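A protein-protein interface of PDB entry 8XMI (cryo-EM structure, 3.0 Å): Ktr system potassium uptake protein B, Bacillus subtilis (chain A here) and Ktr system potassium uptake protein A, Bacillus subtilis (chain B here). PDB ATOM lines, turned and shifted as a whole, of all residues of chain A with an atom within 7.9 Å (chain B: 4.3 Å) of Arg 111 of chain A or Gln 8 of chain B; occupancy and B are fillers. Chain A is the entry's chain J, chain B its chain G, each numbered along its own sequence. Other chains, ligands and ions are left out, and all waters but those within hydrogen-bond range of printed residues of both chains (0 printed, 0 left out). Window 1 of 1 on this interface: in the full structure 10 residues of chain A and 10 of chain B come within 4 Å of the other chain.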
ATOM      1  N   MET A  92      -0.666 -10.723 -10.403  1.00  0.00           N
ATOM      2  CA  MET A  92      -0.449 -11.761  -9.406  1.00  0.00           C
ATOM      3  C   MET A  92       0.337 -11.282  -8.195  1.00  0.00           C
ATOM      4  O   MET A  92       0.350 -11.980  -7.176  1.00  0.00           O
ATOM      5  CB  MET A  92       0.270 -12.957 -10.030  1.00  0.00           C
ATOM      6  CG  MET A  92      -0.663 -13.979 -10.646  1.00  0.00           C
ATOM      7  SD  MET A  92      -1.872 -14.627  -9.475  1.00  0.00           S
ATOM      8  CE  MET A  92      -0.804 -15.262  -8.185  1.00  0.00           C
ATOM      9  N   VAL A  96      -1.251 -12.291  -4.352  1.00  0.00           N
ATOM     10  CA  VAL A  96      -0.569 -12.978  -3.259  1.00  0.00           C
ATOM     11  C   VAL A  96      -0.687 -12.180  -1.967  1.00  0.00           C
ATOM     12  O   VAL A  96      -0.931 -12.742  -0.892  1.00  0.00           O
ATOM     13  CB  VAL A  96       0.898 -13.239  -3.639  1.00  0.00           C
ATOM     14  CG1 VAL A  96       1.690 -13.729  -2.444  1.00  0.00           C
ATOM     15  CG2 VAL A  96       0.958 -14.246  -4.757  1.00  0.00           C
ATOM     16  N   LYS A 105      -2.871 -19.774   3.305  1.00  0.00           N
ATOM     17  CA  LYS A 105      -1.548 -20.304   3.005  1.00  0.00           C
ATOM     18  C   LYS A 105      -1.275 -20.266   1.507  1.00  0.00           C
ATOM     19  O   LYS A 105      -2.188 -20.392   0.686  1.00  0.00           O
ATOM     20  CB  LYS A 105      -1.421 -21.734   3.525  1.00  0.00           C
ATOM     21  CG  LYS A 105      -1.701 -21.879   5.010  1.00  0.00           C
ATOM     22  CD  LYS A 105      -1.376 -23.281   5.498  1.00  0.00           C
ATOM     23  CE  LYS A 105      -1.496 -23.382   7.010  1.00  0.00           C
ATOM     24  NZ  LYS A 105      -1.091 -24.724   7.509  1.00  0.00           N
ATOM     25  N   ILE A 106      -0.004 -20.093   1.153  1.00  0.00           N
ATOM     26  CA  ILE A 106       0.415 -20.090  -0.245  1.00  0.00           C
ATOM     27  C   ILE A 106       0.793 -21.517  -0.629  1.00  0.00           C
ATOM     28  O   ILE A 106       1.769 -22.071  -0.123  1.00  0.00           O
ATOM     29  CB  ILE A 106       1.579 -19.121  -0.483  1.00  0.00           C
ATOM     30  CG1 ILE A 106       1.101 -17.675  -0.359  1.00  0.00           C
ATOM     31  CG2 ILE A 106       2.191 -19.342  -1.854  1.00  0.00           C
ATOM     32  CD1 ILE A 106       0.103 -17.278  -1.422  1.00  0.00           C
ATOM     33  N   GLY A 107       0.013 -22.114  -1.524  1.00  0.00           N
ATOM     34  CA  GLY A 107       0.275 -23.461  -1.973  1.00  0.00           C
ATOM     35  C   GLY A 107       1.298 -23.509  -3.086  1.00  0.00           C
ATOM     36  O   GLY A 107       1.834 -22.498  -3.532  1.00  0.00           O
ATOM     37  N   LEU A 108       1.588 -24.733  -3.526  1.00  0.00           N
ATOM     38  CA  LEU A 108       2.488 -24.919  -4.657  1.00  0.00           C
ATOM     39  C   LEU A 108       1.864 -24.405  -5.945  1.00  0.00           C
ATOM     40  O   LEU A 108       2.560 -23.836  -6.791  1.00  0.00           O
ATOM     41  CB  LEU A 108       2.862 -26.394  -4.788  1.00  0.00           C
ATOM     42  CG  LEU A 108       3.697 -26.818  -5.995  1.00  0.00           C
ATOM     43  CD1 LEU A 108       5.067 -26.171  -5.965  1.00  0.00           C
ATOM     44  CD2 LEU A 108       3.815 -28.324  -6.041  1.00  0.00           C
ATOM     45  N   LYS A 109       0.553 -24.603  -6.113  1.00  0.00           N
ATOM     46  CA  LYS A 109      -0.131 -24.122  -7.309  1.00  0.00           C
ATOM     47  C   LYS A 109      -0.131 -22.600  -7.380  1.00  0.00           C
ATOM     48  O   LYS A 109       0.080 -22.023  -8.453  1.00  0.00           O
ATOM     49  CB  LYS A 109      -1.560 -24.657  -7.340  1.00  0.00           C
ATOM     50  CG  LYS A 109      -1.641 -26.165  -7.435  1.00  0.00           C
ATOM     51  CD  LYS A 109      -3.020 -26.681  -7.072  1.00  0.00           C
ATOM     52  CE  LYS A 109      -3.042 -28.201  -7.070  1.00  0.00           C
ATOM     53  NZ  LYS A 109      -4.227 -28.744  -6.354  1.00  0.00           N
ATOM     54  N   GLU A 110      -0.370 -21.935  -6.250  1.00  0.00           N
ATOM     55  CA  GLU A 110      -0.350 -20.478  -6.228  1.00  0.00           C
ATOM     56  C   GLU A 110       1.070 -19.934  -6.313  1.00  0.00           C
ATOM     57  O   GLU A 110       1.268 -18.790  -6.729  1.00  0.00           O
ATOM     58  CB  GLU A 110      -1.043 -19.971  -4.967  1.00  0.00           C
ATOM     59  CG  GLU A 110      -2.419 -20.583  -4.747  1.00  0.00           C
ATOM     60  CD  GLU A 110      -2.978 -20.295  -3.368  1.00  0.00           C
ATOM     61  OE1 GLU A 110      -2.212 -19.833  -2.497  1.00  0.00           O
ATOM     62  OE2 GLU A 110      -4.187 -20.529  -3.156  1.00  0.00           O
ATOM     63  N   ARG A 111       2.064 -20.728  -5.911  1.00  0.00           N
ATOM     64  CA  ARG A 111       3.454 -20.315  -6.055  1.00  0.00           C
ATOM     65  C   ARG A 111       3.949 -20.473  -7.483  1.00  0.00           C
ATOM     66  O   ARG A 111       4.926 -19.826  -7.868  1.00  0.00           O
ATOM     67  CB  ARG A 111       4.345 -21.112  -5.106  1.00  0.00           C
ATOM     68  CG  ARG A 111       5.300 -20.259  -4.303  1.00  0.00           C
ATOM     69  CD  ARG A 111       6.269 -21.089  -3.483  1.00  0.00           C
ATOM     70  NE  ARG A 111       5.604 -22.147  -2.733  1.00  0.00           N
ATOM     71  CZ  ARG A 111       5.823 -23.442  -2.913  1.00  0.00           C
ATOM     72  NH1 ARG A 111       6.706 -23.877  -3.797  1.00  0.00           N
ATOM     73  NH2 ARG A 111       5.144 -24.324  -2.185  1.00  0.00           N
ATOM     74  N   MET A 112       3.304 -21.332  -8.274  1.00  0.00           N
ATOM     75  CA  MET A 112       3.690 -21.486  -9.672  1.00  0.00           C
ATOM     76  C   MET A 112       3.206 -20.318 -10.522  1.00  0.00           C
ATOM     77  O   MET A 112       3.830 -19.995 -11.537  1.00  0.00           O
ATOM     78  CB  MET A 112       3.152 -22.805 -10.223  1.00  0.00           C
ATOM     79  CG  MET A 112       3.897 -24.033  -9.723  1.00  0.00           C
ATOM     80  SD  MET A 112       2.959 -25.562  -9.888  1.00  0.00           S
ATOM     81  CE  MET A 112       2.801 -25.681 -11.664  1.00  0.00           C
ATOM     82  N   LEU A 113       2.096 -19.685 -10.134  1.00  0.00           N
ATOM     83  CA  LEU A 113       1.611 -18.515 -10.858  1.00  0.00           C
ATOM     84  C   LEU A 113       2.576 -17.345 -10.728  1.00  0.00           C
ATOM     85  O   LEU A 113       2.768 -16.582 -11.681  1.00  0.00           O
ATOM     86  CB  LEU A 113       0.230 -18.113 -10.346  1.00  0.00           C
ATOM     87  CG  LEU A 113      -0.892 -19.145 -10.426  1.00  0.00           C
ATOM     88  CD1 LEU A 113      -2.140 -18.616  -9.747  1.00  0.00           C
ATOM     89  CD2 LEU A 113      -1.186 -19.499 -11.867  1.00  0.00           C
ATOM     90  N   VAL A 114       3.180 -17.182  -9.550  1.00  0.00           N
ATOM     91  CA  VAL A 114       4.130 -16.097  -9.327  1.00  0.00           C
ATOM     92  C   VAL A 114       5.401 -16.324 -10.130  1.00  0.00           C
ATOM     93  O   VAL A 114       6.011 -15.375 -10.635  1.00  0.00           O
ATOM     94  CB  VAL A 114       4.431 -15.967  -7.828  1.00  0.00           C
ATOM     95  CG1 VAL A 114       5.214 -14.706  -7.561  1.00  0.00           C
ATOM     96  CG2 VAL A 114       3.149 -15.983  -7.037  1.00  0.00           C
ATOM     97  N   GLN A 115       5.830 -17.581 -10.245  1.00  0.00           N
ATOM     98  CA  GLN A 115       7.003 -17.902 -11.049  1.00  0.00           C
ATOM     99  C   GLN A 115       6.773 -17.562 -12.515  1.00  0.00           C
ATOM    100  O   GLN A 115       7.686 -17.095 -13.204  1.00  0.00           O
ATOM    101  CB  GLN A 115       7.347 -19.381 -10.885  1.00  0.00           C
ATOM    102  CG  GLN A 115       8.580 -19.819 -11.633  1.00  0.00           C
ATOM    103  CD  GLN A 115       8.673 -21.320 -11.763  1.00  0.00           C
ATOM    104  OE1 GLN A 115       7.792 -22.047 -11.314  1.00  0.00           O
ATOM    105  NE2 GLN A 115       9.740 -21.792 -12.389  1.00  0.00           N
ATOM    106  N   GLU A 116       5.555 -17.792 -13.009  1.00  0.00           N
ATOM    107  CA  GLU A 116       5.232 -17.448 -14.389  1.00  0.00           C
ATOM    108  C   GLU A 116       5.163 -15.937 -14.584  1.00  0.00           C
ATOM    109  O   GLU A 116       5.635 -15.416 -15.602  1.00  0.00           O
ATOM    110  CB  GLU A 116       3.909 -18.102 -14.787  1.00  0.00           C
ATOM    111  CG  GLU A 116       3.536 -17.938 -16.247  1.00  0.00           C
ATOM    112  CD  GLU A 116       4.352 -18.826 -17.167  1.00  0.00           C
ATOM    113  OE1 GLU A 116       4.965 -19.796 -16.673  1.00  0.00           O
ATOM    114  OE2 GLU A 116       4.378 -18.558 -18.387  1.00  0.00           O
ATOM    115  N   ALA A 117       4.583 -15.219 -13.620  1.00  0.00           N
ATOM    116  CA  ALA A 117       4.397 -13.779 -13.767  1.00  0.00           C
ATOM    117  C   ALA A 117       5.719 -13.027 -13.673  1.00  0.00           C
ATOM    118  O   ALA A 117       5.936 -12.051 -14.399  1.00  0.00           O
ATOM    119  CB  ALA A 117       3.415 -13.269 -12.715  1.00  0.00           C
ATOM    120  N   THR A 122      12.945 -20.740 -11.524  1.00  0.00           N
ATOM    121  CA  THR A 122      12.793 -21.649 -10.399  1.00  0.00           C
ATOM    122  C   THR A 122      11.828 -21.047  -9.389  1.00  0.00           C
ATOM    123  O   THR A 122      11.612 -19.835  -9.352  1.00  0.00           O
ATOM    124  CB  THR A 122      14.140 -21.941  -9.723  1.00  0.00           C
ATOM    125  OG1 THR A 122      14.761 -20.710  -9.335  1.00  0.00           O
ATOM    126  CG2 THR A 122      15.069 -22.697 -10.662  1.00  0.00           C
ATOM    127  N   ILE A 123      11.305 -21.841  -8.479  1.00  0.00           N
ATOM    128  CA  ILE A 123      10.348 -21.354  -7.528  1.00  0.00           C
ATOM    129  C   ILE A 123      11.034 -21.109  -6.206  1.00  0.00           C
ATOM    130  O   ILE A 123      10.385 -20.888  -5.201  1.00  0.00           O
ATOM    131  CB  ILE A 123       9.184 -22.342  -7.397  1.00  0.00           C
ATOM    132  CG1 ILE A 123       7.851 -21.615  -7.277  1.00  0.00           C
ATOM    133  CG2 ILE A 123       9.372 -23.260  -6.205  1.00  0.00           C
ATOM    134  CD1 ILE A 123       6.680 -22.563  -7.390  1.00  0.00           C
ATOM    135  N   GLY A 124      12.357 -21.092  -6.204  1.00  0.00           N
ATOM    136  CA  GLY A 124      13.080 -20.847  -4.968  1.00  0.00           C
ATOM    137  C   GLY A 124      13.009 -19.385  -4.570  1.00  0.00           C
ATOM    138  O   GLY A 124      13.612 -18.520  -5.216  1.00  0.00           O
ATOM    139  N   GLY A 125      12.278 -19.104  -3.496  1.00  0.00           N
ATOM    140  CA  GLY A 125      12.149 -17.740  -3.010  1.00  0.00           C
ATOM    141  C   GLY A 125      11.403 -16.818  -3.947  1.00  0.00           C
ATOM    142  O   GLY A 125      11.806 -15.664  -4.132  1.00  0.00           O
ATOM    143  N   VAL A 126      10.285 -17.233  -4.507  1.00  0.00           N
ATOM    144  CA  VAL A 126       9.540 -16.414  -5.438  1.00  0.00           C
ATOM    145  C   VAL A 126       8.469 -15.671  -4.690  1.00  0.00           C
ATOM    146  O   VAL A 126       7.942 -14.697  -5.210  1.00  0.00           O
ATOM    147  CB  VAL A 126       8.888 -17.234  -6.549  1.00  0.00           C
ATOM    148  CG1 VAL A 126       7.618 -17.901  -6.052  1.00  0.00           C
ATOM    149  CG2 VAL A 126       8.587 -16.364  -7.755  1.00  0.00           C
ATOM    150  N   ILE A 127       8.129 -16.082  -3.485  1.00  0.00           N
ATOM    151  CA  ILE A 127       7.196 -15.328  -2.659  1.00  0.00           C
ATOM    152  C   ILE A 127       7.911 -14.255  -1.848  1.00  0.00           C
ATOM    153  O   ILE A 127       7.403 -13.142  -1.700  1.00  0.00           O
ATOM    154  CB  ILE A 127       6.400 -16.288  -1.747  1.00  0.00           C
ATOM    155  CG1 ILE A 127       5.387 -17.073  -2.575  1.00  0.00           C
ATOM    156  CG2 ILE A 127       5.676 -15.538  -0.644  1.00  0.00           C
ATOM    157  CD1 ILE A 127       4.407 -16.203  -3.315  1.00  0.00           C
ATOM    158  N   GLY A 128       9.105 -14.564  -1.340  1.00  0.00           N
ATOM    159  CA  GLY A 128       9.906 -13.562  -0.660  1.00  0.00           C
ATOM    160  C   GLY A 128      10.324 -12.411  -1.545  1.00  0.00           C
ATOM    161  O   GLY A 128      10.585 -11.316  -1.038  1.00  0.00           O
ATOM    162  N   LYS B   7      -1.814 -29.083   3.055  1.00  0.00           N
ATOM    163  CA  LYS B   7      -0.667 -29.980   3.106  1.00  0.00           C
ATOM    164  C   LYS B   7       0.061 -30.033   1.773  1.00  0.00           C
ATOM    165  O   LYS B   7      -0.537 -30.323   0.738  1.00  0.00           O
ATOM    166  CB  LYS B   7      -1.098 -31.389   3.510  1.00  0.00           C
ATOM    167  CG  LYS B   7      -1.327 -31.580   4.995  1.00  0.00           C
ATOM    168  CD  LYS B   7      -1.726 -33.012   5.288  1.00  0.00           C
ATOM    169  CE  LYS B   7      -1.978 -33.229   6.763  1.00  0.00           C
ATOM    170  NZ  LYS B   7      -0.774 -32.920   7.571  1.00  0.00           N
ATOM    171  N   GLN B   8       1.359 -29.758   1.812  1.00  0.00           N
ATOM    172  CA  GLN B   8       2.219 -29.792   0.639  1.00  0.00           C
ATOM    173  C   GLN B   8       3.209 -30.934   0.785  1.00  0.00           C
ATOM    174  O   GLN B   8       3.845 -31.077   1.832  1.00  0.00           O
ATOM    175  CB  GLN B   8       2.970 -28.474   0.469  1.00  0.00           C
ATOM    176  CG  GLN B   8       2.124 -27.299   0.047  1.00  0.00           C
ATOM    177  CD  GLN B   8       2.946 -26.040  -0.075  1.00  0.00           C
ATOM    178  OE1 GLN B   8       3.668 -25.851  -1.051  1.00  0.00           O
ATOM    179  NE2 GLN B   8       2.857 -25.177   0.928  1.00  0.00           N
ATOM    180  N   PHE B   9       3.336 -31.740  -0.264  1.00  0.00           N
ATOM    181  CA  PHE B   9       4.186 -32.918  -0.256  1.00  0.00           C
ATOM    182  C   PHE B   9       5.228 -32.819  -1.356  1.00  0.00           C
ATOM    183  O   PHE B   9       4.942 -32.339  -2.454  1.00  0.00           O
ATOM    184  CB  PHE B   9       3.363 -34.194  -0.450  1.00  0.00           C
ATOM    185  CG  PHE B   9       2.240 -34.343   0.524  1.00  0.00           C
ATOM    186  CD1 PHE B   9       2.461 -34.871   1.777  1.00  0.00           C
ATOM    187  CD2 PHE B   9       0.962 -33.964   0.183  1.00  0.00           C
ATOM    188  CE1 PHE B   9       1.434 -35.007   2.673  1.00  0.00           C
ATOM    189  CE2 PHE B   9      -0.068 -34.103   1.076  1.00  0.00           C
ATOM    190  CZ  PHE B   9       0.169 -34.625   2.323  1.00  0.00           C
ATOM    191  N   GLU B  31      -1.254 -31.392  -3.242  1.00  0.00           N
ATOM    192  CA  GLU B  31      -0.208 -30.730  -4.013  1.00  0.00           C
ATOM    193  C   GLU B  31       1.092 -31.497  -3.832  1.00  0.00           C
ATOM    194  O   GLU B  31       1.726 -31.413  -2.779  1.00  0.00           O
ATOM    195  CB  GLU B  31      -0.049 -29.280  -3.567  1.00  0.00           C
ATOM    196  CG  GLU B  31      -1.272 -28.414  -3.797  1.00  0.00           C
ATOM    197  CD  GLU B  31      -1.236 -27.132  -2.992  1.00  0.00           C
ATOM    198  OE1 GLU B  31      -0.372 -27.014  -2.098  1.00  0.00           O
ATOM    199  OE2 GLU B  31      -2.074 -26.244  -3.247  1.00  0.00           O
ATOM    200  N   GLY B  67      12.145 -25.098  -3.849  1.00  0.00           N
ATOM    201  CA  GLY B  67      11.282 -24.360  -2.951  1.00  0.00           C
ATOM    202  C   GLY B  67      10.973 -25.369  -1.948  1.00  0.00           C
ATOM    203  O   GLY B  67       9.817 -25.581  -1.627  1.00  0.00           O
ATOM    204  N   ASN B  70       9.042 -24.905   1.730  1.00  0.00           N
ATOM    205  CA  ASN B  70       7.606 -24.678   1.775  1.00  0.00           C
ATOM    206  C   ASN B  70       6.809 -25.958   1.980  1.00  0.00           C
ATOM    207  O   ASN B  70       5.583 -25.892   2.104  1.00  0.00           O
ATOM    208  CB  ASN B  70       7.144 -23.997   0.486  1.00  0.00           C
ATOM    209  CG  ASN B  70       7.785 -22.644   0.280  1.00  0.00           C
ATOM    210  OD1 ASN B  70       8.900 -22.545  -0.225  1.00  0.00           O
ATOM    211  ND2 ASN B  70       7.077 -21.591   0.666  1.00  0.00           N
ATOM    212  N   PHE B  71       7.469 -27.108   2.028  1.00  0.00           N
ATOM    213  CA  PHE B  71       6.802 -28.398   2.106  1.00  0.00           C
ATOM    214  C   PHE B  71       6.887 -28.935   3.524  1.00  0.00           C
ATOM    215  O   PHE B  71       7.973 -28.991   4.110  1.00  0.00           O
ATOM    216  CB  PHE B  71       7.420 -29.384   1.117  1.00  0.00           C
ATOM    217  CG  PHE B  71       7.286 -28.960  -0.313  1.00  0.00           C
ATOM    218  CD1 PHE B  71       6.089 -29.114  -0.983  1.00  0.00           C
ATOM    219  CD2 PHE B  71       8.352 -28.405  -0.987  1.00  0.00           C
ATOM    220  CE1 PHE B  71       5.956 -28.724  -2.292  1.00  0.00           C
ATOM    221  CE2 PHE B  71       8.223 -28.013  -2.300  1.00  0.00           C
ATOM    222  CZ  PHE B  71       7.024 -28.175  -2.949  1.00  0.00           C
ATOM    223  N   GLU B  72       5.734 -29.306   4.081  1.00  0.00           N
ATOM    224  CA  GLU B  72       5.701 -29.866   5.426  1.00  0.00           C
ATOM    225  C   GLU B  72       6.206 -31.302   5.441  1.00  0.00           C
ATOM    226  O   GLU B  72       6.956 -31.692   6.342  1.00  0.00           O
ATOM    227  CB  GLU B  72       4.281 -29.795   5.980  1.00  0.00           C
ATOM    228  CG  GLU B  72       3.534 -28.536   5.582  1.00  0.00           C
ATOM    229  CD  GLU B  72       2.164 -28.446   6.218  1.00  0.00           C
ATOM    230  OE1 GLU B  72       1.871 -29.260   7.119  1.00  0.00           O
ATOM    231  OE2 GLU B  72       1.381 -27.559   5.818  1.00  0.00           O
ATOM    232  N   TYR B  73       5.805 -32.102   4.457  1.00  0.00           N
ATOM    233  CA  TYR B  73       6.203 -33.498   4.350  1.00  0.00           C
ATOM    234  C   TYR B  73       7.109 -33.663   3.143  1.00  0.00           C
ATOM    235  O   TYR B  73       6.763 -33.231   2.041  1.00  0.00           O
ATOM    236  CB  TYR B  73       4.988 -34.412   4.216  1.00  0.00           C
ATOM    237  CG  TYR B  73       4.146 -34.534   5.458  1.00  0.00           C
ATOM    238  CD1 TYR B  73       3.132 -33.630   5.723  1.00  0.00           C
ATOM    239  CD2 TYR B  73       4.357 -35.568   6.358  1.00  0.00           C
ATOM    240  CE1 TYR B  73       2.360 -33.743   6.852  1.00  0.00           C
ATOM    241  CE2 TYR B  73       3.589 -35.689   7.489  1.00  0.00           C
ATOM    242  CZ  TYR B  73       2.592 -34.775   7.733  1.00  0.00           C
ATOM    243  OH  TYR B  73       1.820 -34.890   8.863  1.00  0.00           O
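NE2 of Gln 8 of chain B lies within hydrogen-bond range of O of Asn 70 of chain B, at 3.1 Å.
O of Gln 8 of chain B is in hydrogen-bond range of N of Glu 72 of chain B, at 3.4 Å.
The backbone carbonyl oxygen of Gln 8 of chain B is in hydrogen-bond range of the backbone NH of Tyr 73 of chain B (3.4 Å).
The backbone carbonyl oxygen of Glu 31 of chain B sits at hydrogen-bond distance from the backbone NH of Phe 9 of chain B (3.0 Å).
The backbone carbonyl oxygen (O) of Gly 67 of chain B lies close to the side-chain amide oxygen (OD1) of Asn 70 of chain B, at 3.5 Å.
The backbone NH (N) of Gly 107 of chain A is in hydrogen-bond range of the side-chain carboxylate (OE1) of Glu 110 of chain A, 3.3 Å away.
Among the printed residues, merely in contact across the chains: Gly 107 of chain A with Gln 8 of chain B (3.9 Å), Gly 107 of chain A with Glu 31 of chain B (3.6 Å), Lys 109 of chain A with Glu 31 of chain B (3.7 Å), Arg 111 of chain A with Asn 70 of chain B (3.4 Å) and Ile 123 of chain A with Gly 67 of chain B (3.9 Å).
Printed residues of chain B within 4 Å of Gly 107 of chain A: Gln 8 (3.9 Å) and Glu 31 (3.6 Å).
Of the printed residues of chain B, Lys 109 of chain A touches Glu 31.
Arg 111 of chain A touches just these residues of chain B: Gln 8 (2.4 Å) and Asn 70 (3.4 Å).
Val 126 of chain A touches none of the printed residues of chain B.
Of chain A, only Ile 106 (3.5 Å), Gly 107 (3.9 Å), Leu 108 (3.4 Å) and Arg 111 (2.4 Å) come within 4 Å of Gln 8 of chain B.
Printed residues of chain A within 4 Å of Glu 31 of chain B: Gly 107 (3.6 Å), Leu 108 (3.3 Å) and Lys 109 (3.7 Å).
Of the printed residues of chain A, Gly 67 of chain B touches Ile 123 (3.9 Å).
Printed residues of chain A within 4 Å of Asn 70 of chain B: Arg 111 (3.4 Å).
Phe 71 of chain B touches none of the printed residues of chain A.
The nearest printed residue of chain A that does not touch Gln 8 of chain B is Lys 109 of chain A (6.1 Å).
The side-chain amide nitrogen (NE2) of Gln 8 of chain B lies within hydrogen-bond range of the backbone carbonyl oxygen (O) of Ile 106 of chain A, 3.5 Å away.
The backbone NH (N) of Leu 108 of chain A is in hydrogen-bond range of the side-chain amide oxygen (OE1) of Gln 8 of chain B, at 3.4 Å.
The side-chain amide oxygen of Gln 8 of chain B sits at hydrogen-bond distance from the guanidinium group of Arg 111 of chain A (2.4 Å).
OE1 of Glu 31 of chain B sits at hydrogen-bond distance from N of Leu 108 of chain A, 3.3 Å away.
Hydrophobic or aromatic side chains of chain A that line the printed part of chain B: Leu 108 and Ile 123.
Of the 9 printed residues of chain B, 4 touch a printed residue of chain A.
Printed residues of chain B that touch a printed residue of chain A: Gln 8, Glu 31, Gly 67 and Asn 70.
Along chain B the printed residues that touch a printed residue of chain A span positions 8 to 70.
Among the printed residues, 9 pairs touch across the chains.
Among the printed residues, no Asp or Glu carboxylate lies within 4 Å of a Lys or Arg side-chain nitrogen of the other chain.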
